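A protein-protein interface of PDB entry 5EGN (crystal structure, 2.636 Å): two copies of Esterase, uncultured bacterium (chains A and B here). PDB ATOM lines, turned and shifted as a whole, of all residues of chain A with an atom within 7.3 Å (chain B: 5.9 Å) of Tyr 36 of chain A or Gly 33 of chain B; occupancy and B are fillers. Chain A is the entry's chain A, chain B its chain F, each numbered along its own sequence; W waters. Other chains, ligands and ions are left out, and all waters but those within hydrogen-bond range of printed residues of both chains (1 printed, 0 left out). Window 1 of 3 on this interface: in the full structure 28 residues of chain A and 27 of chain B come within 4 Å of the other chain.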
ATOM      1  N   GLY A  32      21.923   6.608  -5.973  1.00  0.00           N
ATOM      2  CA  GLY A  32      23.359   6.638  -5.755  1.00  0.00           C
ATOM      3  C   GLY A  32      24.185   5.842  -6.749  1.00  0.00           C
ATOM      4  O   GLY A  32      25.367   6.136  -6.966  1.00  0.00           O
ATOM      5  N   GLY A  33      23.560   4.842  -7.363  1.00  0.00           N
ATOM      6  CA  GLY A  33      24.230   3.996  -8.334  1.00  0.00           C
ATOM      7  C   GLY A  33      24.937   4.797  -9.412  1.00  0.00           C
ATOM      8  O   GLY A  33      26.026   4.436  -9.847  1.00  0.00           O
ATOM      9  N   ILE A  34      24.324   5.907  -9.819  1.00  0.00           N
ATOM     10  CA  ILE A  34      24.875   6.792 -10.849  1.00  0.00           C
ATOM     11  C   ILE A  34      26.335   7.205 -10.602  1.00  0.00           C
ATOM     12  O   ILE A  34      27.023   7.631 -11.529  1.00  0.00           O
ATOM     13  CB  ILE A  34      24.012   8.078 -10.993  1.00  0.00           C
ATOM     14  CG1 ILE A  34      24.227   8.742 -12.358  1.00  0.00           C
ATOM     15  CG2 ILE A  34      24.297   9.056  -9.859  1.00  0.00           C
ATOM     16  CD1 ILE A  34      23.310   9.917 -12.619  1.00  0.00           C
ATOM     17  N   TRP A  35      26.808   7.066  -9.365  1.00  0.00           N
ATOM     18  CA  TRP A  35      28.173   7.462  -9.033  1.00  0.00           C
ATOM     19  C   TRP A  35      29.167   6.300  -9.084  1.00  0.00           C
ATOM     20  O   TRP A  35      30.264   6.403  -8.522  1.00  0.00           O
ATOM     21  CB  TRP A  35      28.207   8.101  -7.644  1.00  0.00           C
ATOM     22  CG  TRP A  35      27.365   9.329  -7.528  1.00  0.00           C
ATOM     23  CD1 TRP A  35      26.232   9.477  -6.785  1.00  0.00           C
ATOM     24  CD2 TRP A  35      27.585  10.585  -8.183  1.00  0.00           C
ATOM     25  NE1 TRP A  35      25.737  10.750  -6.929  1.00  0.00           N
ATOM     26  CE2 TRP A  35      26.549  11.451  -7.784  1.00  0.00           C
ATOM     27  CE3 TRP A  35      28.559  11.064  -9.067  1.00  0.00           C
ATOM     28  CZ2 TRP A  35      26.456  12.766  -8.234  1.00  0.00           C
ATOM     29  CZ3 TRP A  35      28.466  12.373  -9.514  1.00  0.00           C
ATOM     30  CH2 TRP A  35      27.422  13.208  -9.096  1.00  0.00           C
ATOM     31  N   TYR A  36      28.790   5.217  -9.767  1.00  0.00           N
ATOM     32  CA  TYR A  36      29.578   3.982  -9.779  1.00  0.00           C
ATOM     33  C   TYR A  36      31.024   4.211 -10.204  1.00  0.00           C
ATOM     34  O   TYR A  36      31.946   3.652  -9.614  1.00  0.00           O
ATOM     35  CB  TYR A  36      28.931   2.928 -10.697  1.00  0.00           C
ATOM     36  CG  TYR A  36      29.720   1.634 -10.764  1.00  0.00           C
ATOM     37  CD1 TYR A  36      29.776   0.778  -9.671  1.00  0.00           C
ATOM     38  CD2 TYR A  36      30.431   1.283 -11.906  1.00  0.00           C
ATOM     39  CE1 TYR A  36      30.509  -0.392  -9.713  1.00  0.00           C
ATOM     40  CE2 TYR A  36      31.169   0.109 -11.956  1.00  0.00           C
ATOM     41  CZ  TYR A  36      31.201  -0.721 -10.857  1.00  0.00           C
ATOM     42  OH  TYR A  36      31.929  -1.885 -10.897  1.00  0.00           O
ATOM     43  N   PHE A  37      31.226   5.044 -11.216  1.00  0.00           N
ATOM     44  CA  PHE A  37      32.573   5.261 -11.727  1.00  0.00           C
ATOM     45  C   PHE A  37      33.365   6.274 -10.905  1.00  0.00           C
ATOM     46  O   PHE A  37      34.573   6.413 -11.092  1.00  0.00           O
ATOM     47  CB  PHE A  37      32.530   5.712 -13.185  1.00  0.00           C
ATOM     48  CG  PHE A  37      31.985   4.680 -14.126  1.00  0.00           C
ATOM     49  CD1 PHE A  37      32.719   3.548 -14.441  1.00  0.00           C
ATOM     50  CD2 PHE A  37      30.739   4.846 -14.703  1.00  0.00           C
ATOM     51  CE1 PHE A  37      32.213   2.597 -15.312  1.00  0.00           C
ATOM     52  CE2 PHE A  37      30.229   3.903 -15.573  1.00  0.00           C
ATOM     53  CZ  PHE A  37      30.967   2.777 -15.879  1.00  0.00           C
ATOM     54  N   GLN A  38      32.692   6.976  -9.999  1.00  0.00           N
ATOM     55  CA  GLN A  38      33.364   7.943  -9.136  1.00  0.00           C
ATOM     56  C   GLN A  38      33.632   7.358  -7.756  1.00  0.00           C
ATOM     57  O   GLN A  38      34.702   7.555  -7.181  1.00  0.00           O
ATOM     58  CB  GLN A  38      32.532   9.220  -8.999  1.00  0.00           C
ATOM     59  CG  GLN A  38      32.546  10.122 -10.221  1.00  0.00           C
ATOM     60  CD  GLN A  38      31.699   9.590 -11.357  1.00  0.00           C
ATOM     61  OE1 GLN A  38      30.559   9.175 -11.155  1.00  0.00           O
ATOM     62  NE2 GLN A  38      32.255   9.598 -12.563  1.00  0.00           N
ATOM     63  N   THR A  39      32.645   6.627  -7.249  1.00  0.00           N
ATOM     64  CA  THR A  39      32.625   6.148  -5.870  1.00  0.00           C
ATOM     65  C   THR A  39      33.902   5.441  -5.421  1.00  0.00           C
ATOM     66  O   THR A  39      34.468   5.773  -4.382  1.00  0.00           O
ATOM     67  CB  THR A  39      31.442   5.186  -5.650  1.00  0.00           C
ATOM     68  OG1 THR A  39      30.213   5.875  -5.903  1.00  0.00           O
ATOM     69  CG2 THR A  39      31.437   4.657  -4.225  1.00  0.00           C
ATOM     70  N   PHE A  40      34.358   4.478  -6.211  1.00  0.00           N
ATOM     71  CA  PHE A  40      35.449   3.607  -5.785  1.00  0.00           C
ATOM     72  C   PHE A  40      36.860   4.115  -6.119  1.00  0.00           C
ATOM     73  O   PHE A  40      37.776   3.917  -5.320  1.00  0.00           O
ATOM     74  CB  PHE A  40      35.231   2.207  -6.365  1.00  0.00           C
ATOM     75  CG  PHE A  40      33.923   1.592  -5.955  1.00  0.00           C
ATOM     76  CD1 PHE A  40      33.795   0.964  -4.727  1.00  0.00           C
ATOM     77  CD2 PHE A  40      32.816   1.665  -6.783  1.00  0.00           C
ATOM     78  CE1 PHE A  40      32.591   0.408  -4.339  1.00  0.00           C
ATOM     79  CE2 PHE A  40      31.609   1.111  -6.400  1.00  0.00           C
ATOM     80  CZ  PHE A  40      31.496   0.482  -5.175  1.00  0.00           C
ATOM     81  N   PRO A  41      37.056   4.752  -7.291  1.00  0.00           N
ATOM     82  CA  PRO A  41      38.371   5.378  -7.474  1.00  0.00           C
ATOM     83  C   PRO A  41      38.664   6.452  -6.427  1.00  0.00           C
ATOM     84  O   PRO A  41      39.799   6.557  -5.961  1.00  0.00           O
ATOM     85  CB  PRO A  41      38.271   5.990  -8.872  1.00  0.00           C
ATOM     86  CG  PRO A  41      37.324   5.101  -9.584  1.00  0.00           C
ATOM     87  CD  PRO A  41      36.298   4.710  -8.556  1.00  0.00           C
ATOM     88  N   VAL A  50      28.007   8.213  -0.552  1.00  0.00           N
ATOM     89  CA  VAL A  50      27.051   8.400  -1.639  1.00  0.00           C
ATOM     90  C   VAL A  50      25.633   8.196  -1.117  1.00  0.00           C
ATOM     91  O   VAL A  50      25.347   7.181  -0.467  1.00  0.00           O
ATOM     92  CB  VAL A  50      27.347   7.442  -2.810  1.00  0.00           C
ATOM     93  CG1 VAL A  50      27.634   6.049  -2.294  1.00  0.00           C
ATOM     94  CG2 VAL A  50      26.206   7.434  -3.816  1.00  0.00           C
ATOM     95  N   ARG A  58      16.756   3.389  -2.481  1.00  0.00           N
ATOM     96  CA  ARG A  58      16.664   2.502  -1.329  1.00  0.00           C
ATOM     97  C   ARG A  58      16.210   3.222  -0.065  1.00  0.00           C
ATOM     98  O   ARG A  58      16.016   2.599   0.978  1.00  0.00           O
ATOM     99  CB  ARG A  58      18.017   1.836  -1.090  1.00  0.00           C
ATOM    100  CG  ARG A  58      18.540   1.084  -2.296  1.00  0.00           C
ATOM    101  CD  ARG A  58      20.012   0.768  -2.139  1.00  0.00           C
ATOM    102  NE  ARG A  58      20.866   1.829  -2.658  1.00  0.00           N
ATOM    103  CZ  ARG A  58      21.793   1.645  -3.590  1.00  0.00           C
ATOM    104  NH1 ARG A  58      21.986   0.438  -4.101  1.00  0.00           N
ATOM    105  NH2 ARG A  58      22.530   2.663  -4.010  1.00  0.00           N
ATOM    106  N   GLN A 245      29.314  12.772 -15.344  1.00  0.00           N
ATOM    107  CA  GLN A 245      29.938  11.677 -14.608  1.00  0.00           C
ATOM    108  C   GLN A 245      29.699  10.329 -15.286  1.00  0.00           C
ATOM    109  O   GLN A 245      30.384   9.351 -14.992  1.00  0.00           O
ATOM    110  CB  GLN A 245      29.430  11.634 -13.163  1.00  0.00           C
ATOM    111  CG  GLN A 245      28.050  11.023 -12.983  1.00  0.00           C
ATOM    112  CD  GLN A 245      26.933  12.034 -13.134  1.00  0.00           C
ATOM    113  OE1 GLN A 245      26.844  12.732 -14.142  1.00  0.00           O
ATOM    114  NE2 GLN A 245      26.076  12.123 -12.123  1.00  0.00           N
ATOM    115  N   LEU A 246      28.733  10.284 -16.198  1.00  0.00           N
ATOM    116  CA  LEU A 246      28.446   9.062 -16.945  1.00  0.00           C
ATOM    117  C   LEU A 246      28.866   9.170 -18.409  1.00  0.00           C
ATOM    118  O   LEU A 246      29.305   8.188 -19.009  1.00  0.00           O
ATOM    119  CB  LEU A 246      26.958   8.716 -16.862  1.00  0.00           C
ATOM    120  CG  LEU A 246      26.489   7.987 -15.604  1.00  0.00           C
ATOM    121  CD1 LEU A 246      25.020   7.615 -15.728  1.00  0.00           C
ATOM    122  CD2 LEU A 246      27.339   6.752 -15.357  1.00  0.00           C
ATOM    123  N   ASN A 253      36.302  12.654 -13.412  1.00  0.00           N
ATOM    124  CA  ASN A 253      37.166  12.214 -12.321  1.00  0.00           C
ATOM    125  C   ASN A 253      38.421  13.069 -12.196  1.00  0.00           C
ATOM    126  O   ASN A 253      38.888  13.336 -11.090  1.00  0.00           O
ATOM    127  CB  ASN A 253      37.558  10.747 -12.509  1.00  0.00           C
ATOM    128  CG  ASN A 253      36.449   9.789 -12.121  1.00  0.00           C
ATOM    129  OD1 ASN A 253      35.295  10.183 -11.973  1.00  0.00           O
ATOM    130  ND2 ASN A 253      36.800   8.520 -11.947  1.00  0.00           N
ATOM    131  N   THR B  30      34.256  -7.235  -7.150  1.00  0.00           N
ATOM    132  CA  THR B  30      33.379  -6.092  -7.402  1.00  0.00           C
ATOM    133  C   THR B  30      32.128  -6.171  -6.532  1.00  0.00           C
ATOM    134  O   THR B  30      32.133  -6.822  -5.488  1.00  0.00           O
ATOM    135  CB  THR B  30      32.962  -6.005  -8.882  1.00  0.00           C
ATOM    136  OG1 THR B  30      32.066  -7.079  -9.193  1.00  0.00           O
ATOM    137  CG2 THR B  30      34.181  -6.088  -9.781  1.00  0.00           C
ATOM    138  N   ASN B  31      31.065  -5.497  -6.961  1.00  0.00           N
ATOM    139  CA  ASN B  31      29.771  -5.593  -6.290  1.00  0.00           C
ATOM    140  C   ASN B  31      28.615  -5.301  -7.241  1.00  0.00           C
ATOM    141  O   ASN B  31      28.824  -5.082  -8.432  1.00  0.00           O
ATOM    142  CB  ASN B  31      29.702  -4.652  -5.086  1.00  0.00           C
ATOM    143  CG  ASN B  31      29.924  -3.202  -5.462  1.00  0.00           C
ATOM    144  OD1 ASN B  31      29.057  -2.557  -6.054  1.00  0.00           O
ATOM    145  ND2 ASN B  31      31.086  -2.673  -5.103  1.00  0.00           N
ATOM    146  N   GLY B  32      27.400  -5.289  -6.697  1.00  0.00           N
ATOM    147  CA  GLY B  32      26.187  -5.163  -7.489  1.00  0.00           C
ATOM    148  C   GLY B  32      26.050  -3.891  -8.304  1.00  0.00           C
ATOM    149  O   GLY B  32      25.312  -3.856  -9.295  1.00  0.00           O
ATOM    150  N   GLY B  33      26.765  -2.846  -7.895  1.00  0.00           N
ATOM    151  CA  GLY B  33      26.739  -1.578  -8.601  1.00  0.00           C
ATOM    152  C   GLY B  33      27.062  -1.747 -10.075  1.00  0.00           C
ATOM    153  O   GLY B  33      26.505  -1.056 -10.923  1.00  0.00           O
ATOM    154  N   ILE B  34      27.953  -2.690 -10.374  1.00  0.00           N
ATOM    155  CA  ILE B  34      28.363  -2.993 -11.748  1.00  0.00           C
ATOM    156  C   ILE B  34      27.187  -3.295 -12.692  1.00  0.00           C
ATOM    157  O   ILE B  34      27.328  -3.183 -13.910  1.00  0.00           O
ATOM    158  CB  ILE B  34      29.352  -4.195 -11.779  1.00  0.00           C
ATOM    159  CG1 ILE B  34      30.181  -4.202 -13.068  1.00  0.00           C
ATOM    160  CG2 ILE B  34      28.613  -5.516 -11.612  1.00  0.00           C
ATOM    161  CD1 ILE B  34      31.235  -5.293 -13.108  1.00  0.00           C
ATOM    162  N   TRP B  35      26.034  -3.664 -12.140  1.00  0.00           N
ATOM    163  CA  TRP B  35      24.869  -3.962 -12.967  1.00  0.00           C
ATOM    164  C   TRP B  35      23.988  -2.737 -13.207  1.00  0.00           C
ATOM    165  O   TRP B  35      22.832  -2.887 -13.614  1.00  0.00           O
ATOM    166  CB  TRP B  35      24.028  -5.071 -12.328  1.00  0.00           C
ATOM    167  CG  TRP B  35      24.743  -6.374 -12.177  1.00  0.00           C
ATOM    168  CD1 TRP B  35      25.151  -6.952 -11.011  1.00  0.00           C
ATOM    169  CD2 TRP B  35      25.140  -7.266 -13.228  1.00  0.00           C
ATOM    170  NE1 TRP B  35      25.771  -8.149 -11.269  1.00  0.00           N
ATOM    171  CE2 TRP B  35      25.778  -8.365 -12.621  1.00  0.00           C
ATOM    172  CE3 TRP B  35      25.014  -7.242 -14.621  1.00  0.00           C
ATOM    173  CZ2 TRP B  35      26.291  -9.431 -13.359  1.00  0.00           C
ATOM    174  CZ3 TRP B  35      25.524  -8.304 -15.352  1.00  0.00           C
ATOM    175  CH2 TRP B  35      26.155  -9.383 -14.718  1.00  0.00           C
ATOM    176  N   TYR B  36      24.536  -1.543 -12.963  1.00  0.00           N
ATOM    177  CA  TYR B  36      23.756  -0.299 -12.982  1.00  0.00           C
ATOM    178  C   TYR B  36      22.966  -0.112 -14.269  1.00  0.00           C
ATOM    179  O   TYR B  36      21.797   0.268 -14.235  1.00  0.00           O
ATOM    180  CB  TYR B  36      24.663   0.925 -12.761  1.00  0.00           C
ATOM    181  CG  TYR B  36      23.915   2.248 -12.830  1.00  0.00           C
ATOM    182  CD1 TYR B  36      23.040   2.625 -11.818  1.00  0.00           C
ATOM    183  CD2 TYR B  36      24.065   3.105 -13.916  1.00  0.00           C
ATOM    184  CE1 TYR B  36      22.340   3.819 -11.881  1.00  0.00           C
ATOM    185  CE2 TYR B  36      23.368   4.303 -13.986  1.00  0.00           C
ATOM    186  CZ  TYR B  36      22.508   4.652 -12.964  1.00  0.00           C
ATOM    187  OH  TYR B  36      21.814   5.838 -13.024  1.00  0.00           O
ATOM    188  N   PHE B  37      23.597  -0.388 -15.403  1.00  0.00           N
ATOM    189  CA  PHE B  37      22.944  -0.162 -16.686  1.00  0.00           C
ATOM    190  C   PHE B  37      22.007  -1.296 -17.093  1.00  0.00           C
ATOM    191  O   PHE B  37      21.273  -1.170 -18.072  1.00  0.00           O
ATOM    192  CB  PHE B  37      23.983   0.055 -17.783  1.00  0.00           C
ATOM    193  CG  PHE B  37      24.717   1.359 -17.673  1.00  0.00           C
ATOM    194  CD1 PHE B  37      24.113   2.549 -18.048  1.00  0.00           C
ATOM    195  CD2 PHE B  37      26.015   1.392 -17.198  1.00  0.00           C
ATOM    196  CE1 PHE B  37      24.795   3.748 -17.948  1.00  0.00           C
ATOM    197  CE2 PHE B  37      26.702   2.586 -17.095  1.00  0.00           C
ATOM    198  CZ  PHE B  37      26.090   3.765 -17.471  1.00  0.00           C
ATOM    199  N   VAL B  50      19.483  -8.023  -7.432  1.00  0.00           N
ATOM    200  CA  VAL B  50      20.933  -7.931  -7.600  1.00  0.00           C
ATOM    201  C   VAL B  50      21.666  -8.140  -6.276  1.00  0.00           C
ATOM    202  O   VAL B  50      21.366  -7.480  -5.281  1.00  0.00           O
ATOM    203  CB  VAL B  50      21.335  -6.575  -8.224  1.00  0.00           C
ATOM    204  CG1 VAL B  50      20.590  -5.433  -7.558  1.00  0.00           C
ATOM    205  CG2 VAL B  50      22.839  -6.371  -8.155  1.00  0.00           C
ATOM    206  N   ASP B  52      25.032  -8.618  -3.614  1.00  0.00           N
ATOM    207  CA  ASP B  52      26.420  -8.474  -3.188  1.00  0.00           C
ATOM    208  C   ASP B  52      26.899  -9.761  -2.524  1.00  0.00           C
ATOM    209  O   ASP B  52      26.369 -10.164  -1.489  1.00  0.00           O
ATOM    210  CB  ASP B  52      26.576  -7.301  -2.219  1.00  0.00           C
ATOM    211  CG  ASP B  52      26.616  -5.962  -2.921  1.00  0.00           C
ATOM    212  OD1 ASP B  52      26.196  -5.888  -4.094  1.00  0.00           O
ATOM    213  OD2 ASP B  52      27.069  -4.980  -2.297  1.00  0.00           O
ATOM    214  N   ARG B  58      28.573  -4.321   0.331  1.00  0.00           N
ATOM    215  CA  ARG B  58      27.797  -3.966   1.511  1.00  0.00           C
ATOM    216  C   ARG B  58      27.470  -5.192   2.359  1.00  0.00           C
ATOM    217  O   ARG B  58      26.918  -5.075   3.453  1.00  0.00           O
ATOM    218  CB  ARG B  58      26.512  -3.256   1.090  1.00  0.00           C
ATOM    219  CG  ARG B  58      26.692  -2.329  -0.104  1.00  0.00           C
ATOM    220  CD  ARG B  58      25.369  -2.063  -0.793  1.00  0.00           C
ATOM    221  NE  ARG B  58      25.510  -1.255  -2.001  1.00  0.00           N
ATOM    222  CZ  ARG B  58      25.631  -1.757  -3.225  1.00  0.00           C
ATOM    223  NH1 ARG B  58      25.632  -3.069  -3.410  1.00  0.00           N
ATOM    224  NH2 ARG B  58      25.753  -0.947  -4.267  1.00  0.00           N
ATOM    225  N   VAL B 164      37.819   1.801 -12.413  1.00  0.00           N
ATOM    226  CA  VAL B 164      36.918   1.408 -11.334  1.00  0.00           C
ATOM    227  C   VAL B 164      37.184  -0.035 -10.903  1.00  0.00           C
ATOM    228  O   VAL B 164      37.000  -0.389  -9.733  1.00  0.00           O
ATOM    229  CB  VAL B 164      35.426   1.580 -11.735  1.00  0.00           C
ATOM    230  CG1 VAL B 164      34.998   0.534 -12.748  1.00  0.00           C
ATOM    231  CG2 VAL B 164      34.534   1.515 -10.507  1.00  0.00           C
ATOM    232  N   MET B 165      37.645  -0.861 -11.838  1.00  0.00           N
ATOM    233  CA  MET B 165      37.943  -2.249 -11.512  1.00  0.00           C
ATOM    234  C   MET B 165      39.224  -2.360 -10.692  1.00  0.00           C
ATOM    235  O   MET B 165      39.322  -3.194  -9.793  1.00  0.00           O
ATOM    236  CB  MET B 165      38.050  -3.094 -12.780  1.00  0.00           C
ATOM    237  CG  MET B 165      37.296  -4.408 -12.686  1.00  0.00           C
ATOM    238  SD  MET B 165      35.512  -4.187 -12.528  1.00  0.00           S
ATOM    239  CE  MET B 165      35.120  -3.495 -14.131  1.00  0.00           C
ATOM    240  N   HIS B 168      38.235  -1.318  -7.234  1.00  0.00           N
ATOM    241  CA  HIS B 168      37.475  -2.294  -6.454  1.00  0.00           C
ATOM    242  C   HIS B 168      38.315  -3.085  -5.446  1.00  0.00           C
ATOM    243  O   HIS B 168      37.901  -3.260  -4.299  1.00  0.00           O
ATOM    244  CB  HIS B 168      36.754  -3.268  -7.387  1.00  0.00           C
ATOM    245  CG  HIS B 168      35.396  -2.805  -7.813  1.00  0.00           C
ATOM    246  ND1 HIS B 168      34.390  -2.524  -6.915  1.00  0.00           N
ATOM    247  CD2 HIS B 168      34.874  -2.582  -9.043  1.00  0.00           C
ATOM    248  CE1 HIS B 168      33.309  -2.143  -7.571  1.00  0.00           C
ATOM    249  NE2 HIS B 168      33.576  -2.171  -8.864  1.00  0.00           N
ATOM    250  N   LEU B 246      29.423  -3.730 -19.078  1.00  0.00           N
ATOM    251  CA  LEU B 246      29.980  -2.389 -18.921  1.00  0.00           C
ATOM    252  C   LEU B 246      30.593  -1.863 -20.217  1.00  0.00           C
ATOM    253  O   LEU B 246      30.489  -0.674 -20.521  1.00  0.00           O
ATOM    254  CB  LEU B 246      31.036  -2.367 -17.816  1.00  0.00           C
ATOM    255  CG  LEU B 246      30.559  -2.246 -16.371  1.00  0.00           C
ATOM    256  CD1 LEU B 246      31.753  -2.065 -15.449  1.00  0.00           C
ATOM    257  CD2 LEU B 246      29.581  -1.094 -16.221  1.00  0.00           C
HETATM  258  O   HOH W   1      25.628   1.415  -9.667  1.00  0.00           O
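A ring nitrogen (NE2) of His 168 of chain B is in hydrogen-bond range of the side-chain hydroxyl (OH) of Tyr 36 of chain A.
The side-chain amide oxygen (OD1) of Asn 31 of chain B sits at hydrogen-bond distance from the backbone NH (N) of Gly 33 of chain B (3.0 Å).
Among the printed residues, pairs that only touch across the chains: Phe 40 of chain A with Asn 31 of chain B, Tyr 36 of chain A with Val 164 of chain B, Tyr 36 of chain A with Ile 34 of chain B, Ile 34 of chain A with Tyr 36 of chain B, Gly 33 of chain A with Tyr 36 of chain B, Tyr 36 of chain A with Gly 33 of chain B, Phe 40 of chain A with His 168 of chain B and Leu 246 of chain A with Phe 37 of chain B.
No residue of chain A comes within 4 Å of Gly 32 of chain B.
Of the printed residues of chain B, Phe 40 of chain A touches Asn 31 and His 168.
Of the printed residues of chain A, Tyr 36 of chain B touches Gly 33 and Ile 34.
Arg 58 of chain A touches none of the printed residues of chain B.
The nearest residue of chain B that does not touch Tyr 36 of chain A is Leu 246 of chain B (4.2 Å).
The nearest printed residue of chain A that does not touch Ile 34 of chain B is Phe 40 of chain A (6.6 Å).
Of the 15 printed residues of chain B, 7 touch a printed residue of chain A.
Printed residues of chain B that touch a printed residue of chain A: Asn 31, Gly 33, Ile 34, Tyr 36, Phe 37, Val 164 and His 168.
Hydrophobic or aromatic side chains of chain B that line the printed part of chain A: Ile 34, Tyr 36, Phe 37, Val 164 and His 168.
Printed residues of chain A that touch a printed residue of chain B: Gly 33, Ile 34, Tyr 36, Phe 40 and Leu 246.
Hydrophobic or aromatic side chains of chain A that line the printed part of chain B: Ile 34, Tyr 36, Phe 40 and Leu 246.
Among the printed residues, 9 pairs touch across the chains.
Among the printed residues, no Asp or Glu carboxylate lies within 4 Å of a Lys or Arg side-chain nitrogen of the other chain.
Gly 33 of chain A touches Tyr 36 of chain B, and with the chains exchanged Tyr 36 of chain A touches Gly 33 of chain B.
Ile 34 of chain A touches Tyr 36 of chain B, and with the chains exchanged Tyr 36 of chain A touches Ile 34 of chain B.
Leu 246 of chain A touches Phe 37 of chain B, but with the chains exchanged Phe 37 of chain A does not touch Leu 246 of chain B (4.1 Å).
9 positions are printed for both chains.
Water W1 bridges O of Gly 33 of chain B (2.9 Å) and O of Gly 33 of chain A (3.1 Å).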
